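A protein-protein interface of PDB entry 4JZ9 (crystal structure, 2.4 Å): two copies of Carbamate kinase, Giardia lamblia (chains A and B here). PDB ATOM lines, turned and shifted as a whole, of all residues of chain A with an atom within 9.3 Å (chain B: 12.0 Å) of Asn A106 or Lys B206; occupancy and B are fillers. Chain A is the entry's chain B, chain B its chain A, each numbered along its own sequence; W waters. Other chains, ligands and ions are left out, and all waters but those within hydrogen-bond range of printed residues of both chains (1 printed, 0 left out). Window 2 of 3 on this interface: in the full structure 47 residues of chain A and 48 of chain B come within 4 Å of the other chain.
No position is printed for both chains.
Water W1 bridges the side-chain amide nitrogen (NE2) of Gln A96 (2.9 Å) and the backbone NH (N) of Gly B210 (3.0 Å).
The backbone carbonyl oxygen (O) of Lys B206 lies within hydrogen-bond range of the side-chain sulfur (SG) of Cys A103. The side-chain amino group of Lys B206 is in hydrogen-bond range of the side-chain amide oxygen of Asn A106 (3.2 Å). The side-chain amide nitrogen of Gln B117 lies within hydrogen-bond range of the side-chain carboxylate of Asp A99. The side-chain amide oxygen (OE1) of Gln B117 sits close to the side-chain amide oxygen (OE1) of Gln A96, at 3.4 Å. N of Ile B208 is in hydrogen-bond range of OD1 of Asn A100, 2.9 Å away.
Among the printed residues, pairs that only touch across the chains: Gln A96 with Cys B201, Gln A96 with Ile B208, Gln A96 with Ser B209, Gln A96 with Gly B210, Asp A99 with Val B176, Asn A100 with Lys B206 and Asn A100 with Val B207.
Along chain B the printed residues that touch a printed residue of chain A span positions 117 to 210. Among the printed residues, no Asp or Glu carboxylate lies within 4 Å of a Lys or Arg side-chain nitrogen of the other chain.
Of the printed residues of chain B, Gln A96 touches Gln B117 (3.0 Å), Cys B201 (3.9 Å), Ile B208 (3.3 Å), Ser B209 (3.5 Å) and Gly B210 (3.7 Å). Of the printed residues of chain B, Asp A99 touches Gln B117 (3.3 Å) and Val B176 (3.6 Å). Printed residues of chain B within 4 Å of Asn A100: Lys B206 (3.8 Å), Val B207 (3.7 Å) and Ile B208 (2.9 Å). No residue of chain B comes within 4 Å of Ala A104. Asn A105 touches none of the printed residues of chain B. Asn A106 touches just one residue of chain B: Lys B206. No residue of chain B comes within 4 Å of Glu A107. Ala A109 touches none of the printed residues of chain B. Of the printed residues of chain A, Val B176 touches Asp A99 (3.6 Å). Lys B206 touches three residues of chain A. Val B207 touches just one residue of chain A: Asn A100 (3.7 Å). Of the printed residues of chain A, Ile B208 touches Gln A96 and Asn A100. Printed residues of chain A within 4 Å of Ser B209: Gln A96. The nearest residue of chain B that does not touch Asn A106 is Asn B205 (9.5 Å). The nearest residue of chain A that does not touch Lys B206 is Ala A104 (4.6 Å). The nearest printed residue of chain A that does not touch Gln B117 is Ala A97 (5.9 Å).
N of Lys B202 sits at hydrogen-bond distance from O of Ser B209 (3.0 Å). O of Gln A96 lies within hydrogen-bond range of ND2 of Asn A100. O of Gln B117 is in hydrogen-bond range of N of Val B176 (3.1 Å).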
ATOM      1  N   TYR A  41     -28.105  -0.489 -11.713  1.00  0.00           N
ATOM      2  CA  TYR A  41     -27.071  -1.511 -11.629  1.00  0.00           C
ATOM      3  C   TYR A  41     -27.626  -2.934 -11.783  1.00  0.00           C
ATOM      4  O   TYR A  41     -27.022  -3.787 -12.438  1.00  0.00           O
ATOM      5  CB  TYR A  41     -26.285  -1.386 -10.331  1.00  0.00           C
ATOM      6  CG  TYR A  41     -25.263  -2.475 -10.176  1.00  0.00           C
ATOM      7  CD1 TYR A  41     -24.076  -2.436 -10.892  1.00  0.00           C
ATOM      8  CD2 TYR A  41     -25.491  -3.565  -9.340  1.00  0.00           C
ATOM      9  CE1 TYR A  41     -23.134  -3.435 -10.774  1.00  0.00           C
ATOM     10  CE2 TYR A  41     -24.556  -4.567  -9.211  1.00  0.00           C
ATOM     11  CZ  TYR A  41     -23.374  -4.491  -9.932  1.00  0.00           C
ATOM     12  OH  TYR A  41     -22.422  -5.479  -9.821  1.00  0.00           O
ATOM     13  N   HIS A  44     -27.681  -3.819 -15.340  1.00  0.00           N
ATOM     14  CA  HIS A  44     -26.343  -4.118 -15.817  1.00  0.00           C
ATOM     15  C   HIS A  44     -25.958  -5.494 -15.344  1.00  0.00           C
ATOM     16  O   HIS A  44     -25.431  -6.296 -16.104  1.00  0.00           O
ATOM     17  CB  HIS A  44     -25.346  -3.112 -15.246  1.00  0.00           C
ATOM     18  CG  HIS A  44     -23.928  -3.587 -15.280  1.00  0.00           C
ATOM     19  ND1 HIS A  44     -23.128  -3.477 -16.394  1.00  0.00           N
ATOM     20  CD2 HIS A  44     -23.163  -4.189 -14.332  1.00  0.00           C
ATOM     21  CE1 HIS A  44     -21.937  -3.984 -16.137  1.00  0.00           C
ATOM     22  NE2 HIS A  44     -21.939  -4.424 -14.887  1.00  0.00           N
ATOM     23  N   GLN A  96     -20.306   9.101 -11.064  1.00  0.00           N
ATOM     24  CA  GLN A  96     -19.698   8.873  -9.759  1.00  0.00           C
ATOM     25  C   GLN A  96     -20.588   7.940  -8.938  1.00  0.00           C
ATOM     26  O   GLN A  96     -20.100   7.137  -8.157  1.00  0.00           O
ATOM     27  CB  GLN A  96     -19.428  10.173  -8.980  1.00  0.00           C
ATOM     28  CG  GLN A  96     -19.034   9.883  -7.519  1.00  0.00           C
ATOM     29  CD  GLN A  96     -18.784  11.119  -6.701  1.00  0.00           C
ATOM     30  OE1 GLN A  96     -17.679  11.652  -6.693  1.00  0.00           O
ATOM     31  NE2 GLN A  96     -19.793  11.571  -5.992  1.00  0.00           N
ATOM     32  N   ALA A  97     -21.901   8.070  -9.099  1.00  0.00           N
ATOM     33  CA  ALA A  97     -22.844   7.224  -8.373  1.00  0.00           C
ATOM     34  C   ALA A  97     -22.737   5.790  -8.898  1.00  0.00           C
ATOM     35  O   ALA A  97     -22.478   4.859  -8.143  1.00  0.00           O
ATOM     36  CB  ALA A  97     -24.259   7.753  -8.520  1.00  0.00           C
ATOM     37  N   MET A  98     -22.881   5.649 -10.210  1.00  0.00           N
ATOM     38  CA  MET A  98     -22.699   4.371 -10.859  1.00  0.00           C
ATOM     39  C   MET A  98     -21.393   3.699 -10.496  1.00  0.00           C
ATOM     40  O   MET A  98     -21.353   2.500 -10.228  1.00  0.00           O
ATOM     41  CB  MET A  98     -22.784   4.508 -12.371  1.00  0.00           C
ATOM     42  CG  MET A  98     -23.270   3.222 -13.003  1.00  0.00           C
ATOM     43  SD  MET A  98     -24.890   2.793 -12.293  1.00  0.00           S
ATOM     44  CE  MET A  98     -25.708   4.332 -12.674  1.00  0.00           C
ATOM     45  N   ASP A  99     -20.312   4.456 -10.511  1.00  0.00           N
ATOM     46  CA  ASP A  99     -19.026   3.891 -10.112  1.00  0.00           C
ATOM     47  C   ASP A  99     -19.082   3.335  -8.690  1.00  0.00           C
ATOM     48  O   ASP A  99     -18.410   2.350  -8.380  1.00  0.00           O
ATOM     49  CB  ASP A  99     -17.912   4.931 -10.188  1.00  0.00           C
ATOM     50  CG  ASP A  99     -17.514   5.264 -11.624  1.00  0.00           C
ATOM     51  OD1 ASP A  99     -16.832   6.308 -11.806  1.00  0.00           O
ATOM     52  OD2 ASP A  99     -17.883   4.487 -12.557  1.00  0.00           O
ATOM     53  N   ASN A 100     -19.874   3.959  -7.818  1.00  0.00           N
ATOM     54  CA  ASN A 100     -19.922   3.490  -6.443  1.00  0.00           C
ATOM     55  C   ASN A 100     -20.766   2.210  -6.241  1.00  0.00           C
ATOM     56  O   ASN A 100     -20.385   1.321  -5.475  1.00  0.00           O
ATOM     57  CB  ASN A 100     -20.327   4.621  -5.503  1.00  0.00           C
ATOM     58  CG  ASN A 100     -19.220   5.651  -5.309  1.00  0.00           C
ATOM     59  OD1 ASN A 100     -18.026   5.330  -5.397  1.00  0.00           O
ATOM     60  ND2 ASN A 100     -19.613   6.897  -5.035  1.00  0.00           N
ATOM     61  N   VAL A 101     -21.894   2.091  -6.935  1.00  0.00           N
ATOM     62  CA  VAL A 101     -22.579   0.804  -6.947  1.00  0.00           C
ATOM     63  C   VAL A 101     -21.619  -0.301  -7.455  1.00  0.00           C
ATOM     64  O   VAL A 101     -21.465  -1.336  -6.834  1.00  0.00           O
ATOM     65  CB  VAL A 101     -23.858   0.821  -7.814  1.00  0.00           C
ATOM     66  CG1 VAL A 101     -24.868  -0.133  -7.238  1.00  0.00           C
ATOM     67  CG2 VAL A 101     -24.433   2.210  -7.904  1.00  0.00           C
ATOM     68  N   PHE A 102     -20.969  -0.058  -8.585  1.00  0.00           N
ATOM     69  CA  PHE A 102     -20.018  -1.016  -9.131  1.00  0.00           C
ATOM     70  C   PHE A 102     -19.059  -1.542  -8.067  1.00  0.00           C
ATOM     71  O   PHE A 102     -18.908  -2.750  -7.912  1.00  0.00           O
ATOM     72  CB  PHE A 102     -19.232  -0.403 -10.304  1.00  0.00           C
ATOM     73  CG  PHE A 102     -19.863  -0.646 -11.640  1.00  0.00           C
ATOM     74  CD1 PHE A 102     -21.185  -0.290 -11.872  1.00  0.00           C
ATOM     75  CD2 PHE A 102     -19.146  -1.251 -12.663  1.00  0.00           C
ATOM     76  CE1 PHE A 102     -21.786  -0.532 -13.101  1.00  0.00           C
ATOM     77  CE2 PHE A 102     -19.735  -1.490 -13.893  1.00  0.00           C
ATOM     78  CZ  PHE A 102     -21.064  -1.130 -14.109  1.00  0.00           C
ATOM     79  N   CYS A 103     -18.426  -0.624  -7.339  1.00  0.00           N
ATOM     80  CA  CYS A 103     -17.361  -0.952  -6.381  1.00  0.00           C
ATOM     81  C   CYS A 103     -17.884  -1.617  -5.102  1.00  0.00           C
ATOM     82  O   CYS A 103     -17.259  -2.545  -4.570  1.00  0.00           O
ATOM     83  CB  CYS A 103     -16.559   0.307  -6.048  1.00  0.00           C
ATOM     84  SG  CYS A 103     -15.206   0.115  -4.845  1.00  0.00           S
ATOM     85  N   ALA A 104     -19.025  -1.131  -4.614  1.00  0.00           N
ATOM     86  CA  ALA A 104     -19.737  -1.776  -3.515  1.00  0.00           C
ATOM     87  C   ALA A 104     -19.966  -3.246  -3.839  1.00  0.00           C
ATOM     88  O   ALA A 104     -20.016  -4.076  -2.933  1.00  0.00           O
ATOM     89  CB  ALA A 104     -21.076  -1.084  -3.245  1.00  0.00           C
ATOM     90  N   ASN A 105     -20.091  -3.544  -5.134  1.00  0.00           N
ATOM     91  CA  ASN A 105     -20.292  -4.896  -5.652  1.00  0.00           C
ATOM     92  C   ASN A 105     -19.019  -5.504  -6.220  1.00  0.00           C
ATOM     93  O   ASN A 105     -19.075  -6.429  -7.028  1.00  0.00           O
ATOM     94  CB  ASN A 105     -21.300  -4.865  -6.797  1.00  0.00           C
ATOM     95  CG  ASN A 105     -22.678  -4.533  -6.343  1.00  0.00           C
ATOM     96  OD1 ASN A 105     -23.635  -5.226  -6.675  1.00  0.00           O
ATOM     97  ND2 ASN A 105     -22.794  -3.499  -5.524  1.00  0.00           N
ATOM     98  N   ASN A 106     -17.877  -4.964  -5.824  1.00  0.00           N
ATOM     99  CA  ASN A 106     -16.605  -5.521  -6.221  1.00  0.00           C
ATOM    100  C   ASN A 106     -16.496  -5.870  -7.703  1.00  0.00           C
ATOM    101  O   ASN A 106     -15.958  -6.917  -8.074  1.00  0.00           O
ATOM    102  CB  ASN A 106     -16.288  -6.733  -5.377  1.00  0.00           C
ATOM    103  CG  ASN A 106     -15.213  -6.439  -4.375  1.00  0.00           C
ATOM    104  OD1 ASN A 106     -15.493  -6.003  -3.260  1.00  0.00           O
ATOM    105  ND2 ASN A 106     -13.965  -6.653  -4.769  1.00  0.00           N
ATOM    106  N   GLU A 107     -17.033  -4.998  -8.546  1.00  0.00           N
ATOM    107  CA  GLU A 107     -16.848  -5.095  -9.984  1.00  0.00           C
ATOM    108  C   GLU A 107     -16.176  -3.782 -10.363  1.00  0.00           C
ATOM    109  O   GLU A 107     -16.672  -2.708  -9.998  1.00  0.00           O
ATOM    110  CB  GLU A 107     -18.199  -5.287 -10.677  1.00  0.00           C
ATOM    111  CG  GLU A 107     -18.305  -4.618 -12.042  1.00  0.00           C
ATOM    112  CD  GLU A 107     -19.548  -5.053 -12.829  1.00  0.00           C
ATOM    113  OE1 GLU A 107     -19.541  -4.889 -14.074  1.00  0.00           O
ATOM    114  OE2 GLU A 107     -20.530  -5.558 -12.217  1.00  0.00           O
ATOM    115  N   PRO A 108     -15.027  -3.853 -11.061  1.00  0.00           N
ATOM    116  CA  PRO A 108     -14.275  -2.621 -11.304  1.00  0.00           C
ATOM    117  C   PRO A 108     -14.993  -1.729 -12.295  1.00  0.00           C
ATOM    118  O   PRO A 108     -15.618  -2.214 -13.235  1.00  0.00           O
ATOM    119  CB  PRO A 108     -12.962  -3.125 -11.897  1.00  0.00           C
ATOM    120  CG  PRO A 108     -13.329  -4.356 -12.566  1.00  0.00           C
ATOM    121  CD  PRO A 108     -14.385  -5.006 -11.707  1.00  0.00           C
ATOM    122  N   ALA A 109     -14.894  -0.427 -12.078  1.00  0.00           N
ATOM    123  CA  ALA A 109     -15.659   0.526 -12.856  1.00  0.00           C
ATOM    124  C   ALA A 109     -15.284   0.547 -14.334  1.00  0.00           C
ATOM    125  O   ALA A 109     -14.106   0.503 -14.692  1.00  0.00           O
ATOM    126  CB  ALA A 109     -15.532   1.938 -12.248  1.00  0.00           C
ATOM    127  N   GLN B 117     -13.027  12.323 -13.365  1.00  0.00           N
ATOM    128  CA  GLN B 117     -12.762  12.397 -11.935  1.00  0.00           C
ATOM    129  C   GLN B 117     -11.323  12.010 -11.670  1.00  0.00           C
ATOM    130  O   GLN B 117     -10.818  11.021 -12.248  1.00  0.00           O
ATOM    131  CB  GLN B 117     -13.649  11.382 -11.197  1.00  0.00           C
ATOM    132  CG  GLN B 117     -15.142  11.699 -11.239  1.00  0.00           C
ATOM    133  CD  GLN B 117     -16.010  10.521 -10.821  1.00  0.00           C
ATOM    134  OE1 GLN B 117     -16.518  10.476  -9.687  1.00  0.00           O
ATOM    135  NE2 GLN B 117     -16.195   9.561 -11.741  1.00  0.00           N
ATOM    136  N   LEU B 119      -8.698  10.995  -8.593  1.00  0.00           N
ATOM    137  CA  LEU B 119      -8.501  10.691  -7.183  1.00  0.00           C
ATOM    138  C   LEU B 119      -7.284  11.395  -6.604  1.00  0.00           C
ATOM    139  O   LEU B 119      -6.270  11.540  -7.274  1.00  0.00           O
ATOM    140  CB  LEU B 119      -8.390   9.193  -6.959  1.00  0.00           C
ATOM    141  CG  LEU B 119      -9.712   8.445  -7.178  1.00  0.00           C
ATOM    142  CD1 LEU B 119      -9.571   6.962  -6.814  1.00  0.00           C
ATOM    143  CD2 LEU B 119     -10.891   9.095  -6.440  1.00  0.00           C
ATOM    144  N   PRO B 122      -6.453  12.624   0.753  1.00  0.00           N
ATOM    145  CA  PRO B 122      -7.242  13.495   1.638  1.00  0.00           C
ATOM    146  C   PRO B 122      -6.359  14.188   2.665  1.00  0.00           C
ATOM    147  O   PRO B 122      -6.749  15.159   3.310  1.00  0.00           O
ATOM    148  CB  PRO B 122      -8.196  12.520   2.339  1.00  0.00           C
ATOM    149  CG  PRO B 122      -8.096  11.245   1.576  1.00  0.00           C
ATOM    150  CD  PRO B 122      -6.701  11.208   1.042  1.00  0.00           C
ATOM    151  N   GLU B 174      -4.898   9.278  -9.428  1.00  0.00           N
ATOM    152  CA  GLU B 174      -5.514   8.332 -10.353  1.00  0.00           C
ATOM    153  C   GLU B 174      -6.652   8.950 -11.182  1.00  0.00           C
ATOM    154  O   GLU B 174      -7.469   9.735 -10.664  1.00  0.00           O
ATOM    155  CB  GLU B 174      -6.008   7.094  -9.591  1.00  0.00           C
ATOM    156  CG  GLU B 174      -6.967   6.215 -10.396  1.00  0.00           C
ATOM    157  CD  GLU B 174      -7.253   4.872  -9.720  1.00  0.00           C
ATOM    158  OE1 GLU B 174      -7.861   3.979 -10.374  1.00  0.00           O
ATOM    159  OE2 GLU B 174      -6.870   4.713  -8.534  1.00  0.00           O
ATOM    160  N   VAL B 176      -9.923   8.130 -12.712  1.00  0.00           N
ATOM    161  CA  VAL B 176     -10.950   7.122 -12.512  1.00  0.00           C
ATOM    162  C   VAL B 176     -11.395   6.513 -13.843  1.00  0.00           C
ATOM    163  O   VAL B 176     -11.663   5.318 -13.948  1.00  0.00           O
ATOM    164  CB  VAL B 176     -12.179   7.725 -11.801  1.00  0.00           C
ATOM    165  CG1 VAL B 176     -13.262   6.664 -11.588  1.00  0.00           C
ATOM    166  CG2 VAL B 176     -11.768   8.387 -10.485  1.00  0.00           C
ATOM    167  N   CYS B 201     -11.297  14.108  -6.425  1.00  0.00           N
ATOM    168  CA  CYS B 201     -12.092  13.262  -5.547  1.00  0.00           C
ATOM    169  C   CYS B 201     -11.212  12.496  -4.576  1.00  0.00           C
ATOM    170  O   CYS B 201      -9.983  12.494  -4.694  1.00  0.00           O
ATOM    171  CB  CYS B 201     -12.918  12.259  -6.353  1.00  0.00           C
ATOM    172  SG  CYS B 201     -14.088  13.011  -7.440  1.00  0.00           S
ATOM    173  N   LYS B 202     -11.860  11.853  -3.611  1.00  0.00           N
ATOM    174  CA  LYS B 202     -11.194  10.933  -2.715  1.00  0.00           C
ATOM    175  C   LYS B 202     -12.021   9.672  -2.637  1.00  0.00           C
ATOM    176  O   LYS B 202     -13.216   9.671  -2.937  1.00  0.00           O
ATOM    177  CB  LYS B 202     -11.017  11.533  -1.320  1.00  0.00           C
ATOM    178  CG  LYS B 202     -12.321  11.790  -0.565  1.00  0.00           C
ATOM    179  CD  LYS B 202     -12.106  11.730   0.933  1.00  0.00           C
ATOM    180  CE  LYS B 202     -13.427  11.687   1.693  1.00  0.00           C
ATOM    181  NZ  LYS B 202     -14.332  12.825   1.333  1.00  0.00           N
ATOM    182  N   ARG B 203     -11.366   8.589  -2.255  1.00  0.00           N
ATOM    183  CA  ARG B 203     -12.022   7.309  -2.155  1.00  0.00           C
ATOM    184  C   ARG B 203     -11.639   6.653  -0.842  1.00  0.00           C
ATOM    185  O   ARG B 203     -10.476   6.335  -0.623  1.00  0.00           O
ATOM    186  CB  ARG B 203     -11.614   6.419  -3.325  1.00  0.00           C
ATOM    187  CG  ARG B 203     -12.375   5.090  -3.393  1.00  0.00           C
ATOM    188  CD  ARG B 203     -11.456   3.952  -3.808  1.00  0.00           C
ATOM    189  NE  ARG B 203     -11.309   3.830  -5.252  1.00  0.00           N
ATOM    190  CZ  ARG B 203     -10.161   3.571  -5.885  1.00  0.00           C
ATOM    191  NH1 ARG B 203      -9.014   3.418  -5.211  1.00  0.00           N
ATOM    192  NH2 ARG B 203     -10.164   3.470  -7.211  1.00  0.00           N
ATOM    193  N   GLU B 204     -12.613   6.468   0.040  1.00  0.00           N
ATOM    194  CA  GLU B 204     -12.370   5.708   1.257  1.00  0.00           C
ATOM    195  C   GLU B 204     -13.531   4.770   1.583  1.00  0.00           C
ATOM    196  O   GLU B 204     -14.703   5.128   1.415  1.00  0.00           O
ATOM    197  CB  GLU B 204     -12.069   6.643   2.422  1.00  0.00           C
ATOM    198  CG  GLU B 204     -13.029   7.815   2.542  1.00  0.00           C
ATOM    199  CD  GLU B 204     -12.554   8.850   3.557  1.00  0.00           C
ATOM    200  OE1 GLU B 204     -11.331   9.132   3.563  1.00  0.00           O
ATOM    201  OE2 GLU B 204     -13.397   9.361   4.346  1.00  0.00           O
ATOM    202  N   ASN B 205     -13.201   3.567   2.045  1.00  0.00           N
ATOM    203  CA  ASN B 205     -14.219   2.560   2.323  1.00  0.00           C
ATOM    204  C   ASN B 205     -15.172   2.414   1.141  1.00  0.00           C
ATOM    205  O   ASN B 205     -16.387   2.640   1.278  1.00  0.00           O
ATOM    206  CB  ASN B 205     -14.998   2.911   3.587  1.00  0.00           C
ATOM    207  CG  ASN B 205     -14.213   3.815   4.512  1.00  0.00           C
ATOM    208  OD1 ASN B 205     -14.676   4.907   4.877  1.00  0.00           O
ATOM    209  ND2 ASN B 205     -13.004   3.376   4.886  1.00  0.00           N
ATOM    210  N   LYS B 206     -14.581   2.080  -0.010  1.00  0.00           N
ATOM    211  CA  LYS B 206     -15.289   1.780  -1.263  1.00  0.00           C
ATOM    212  C   LYS B 206     -16.103   2.918  -1.920  1.00  0.00           C
ATOM    213  O   LYS B 206     -16.839   2.692  -2.886  1.00  0.00           O
ATOM    214  CB  LYS B 206     -16.146   0.514  -1.099  1.00  0.00           C
ATOM    215  CG  LYS B 206     -15.364  -0.802  -1.297  1.00  0.00           C
ATOM    216  CD  LYS B 206     -16.000  -1.990  -0.549  1.00  0.00           C
ATOM    217  CE  LYS B 206     -15.796  -3.298  -1.300  1.00  0.00           C
ATOM    218  NZ  LYS B 206     -14.375  -3.464  -1.741  1.00  0.00           N
ATOM    219  N   VAL B 207     -15.955   4.136  -1.414  1.00  0.00           N
ATOM    220  CA  VAL B 207     -16.799   5.242  -1.864  1.00  0.00           C
ATOM    221  C   VAL B 207     -15.986   6.421  -2.379  1.00  0.00           C
ATOM    222  O   VAL B 207     -15.065   6.876  -1.710  1.00  0.00           O
ATOM    223  CB  VAL B 207     -17.752   5.713  -0.742  1.00  0.00           C
ATOM    224  CG1 VAL B 207     -18.622   6.851  -1.220  1.00  0.00           C
ATOM    225  CG2 VAL B 207     -18.609   4.543  -0.247  1.00  0.00           C
ATOM    226  N   ILE B 208     -16.325   6.884  -3.582  1.00  0.00           N
ATOM    227  CA  ILE B 208     -15.719   8.063  -4.193  1.00  0.00           C
ATOM    228  C   ILE B 208     -16.621   9.262  -3.964  1.00  0.00           C
ATOM    229  O   ILE B 208     -17.827   9.177  -4.203  1.00  0.00           O
ATOM    230  CB  ILE B 208     -15.563   7.918  -5.725  1.00  0.00           C
ATOM    231  CG1 ILE B 208     -14.744   6.675  -6.090  1.00  0.00           C
ATOM    232  CG2 ILE B 208     -14.918   9.172  -6.320  1.00  0.00           C
ATOM    233  CD1 ILE B 208     -14.795   6.312  -7.596  1.00  0.00           C
ATOM    234  N   SER B 209     -16.036  10.377  -3.522  1.00  0.00           N
ATOM    235  CA  SER B 209     -16.778  11.619  -3.361  1.00  0.00           C
ATOM    236  C   SER B 209     -15.882  12.838  -3.603  1.00  0.00           C
ATOM    237  O   SER B 209     -14.665  12.787  -3.392  1.00  0.00           O
ATOM    238  CB  SER B 209     -17.446  11.684  -1.987  1.00  0.00           C
ATOM    239  OG  SER B 209     -16.487  11.557  -0.957  1.00  0.00           O
ATOM    240  N   GLY B 210     -16.506  13.928  -4.051  1.00  0.00           N
ATOM    241  CA  GLY B 210     -15.788  15.083  -4.535  1.00  0.00           C
ATOM    242  C   GLY B 210     -15.202  15.862  -3.382  1.00  0.00           C
ATOM    243  O   GLY B 210     -15.860  16.026  -2.353  1.00  0.00           O
HETATM  244  O   HOH W   1     -19.499  13.481  -3.852  1.00  0.00           O
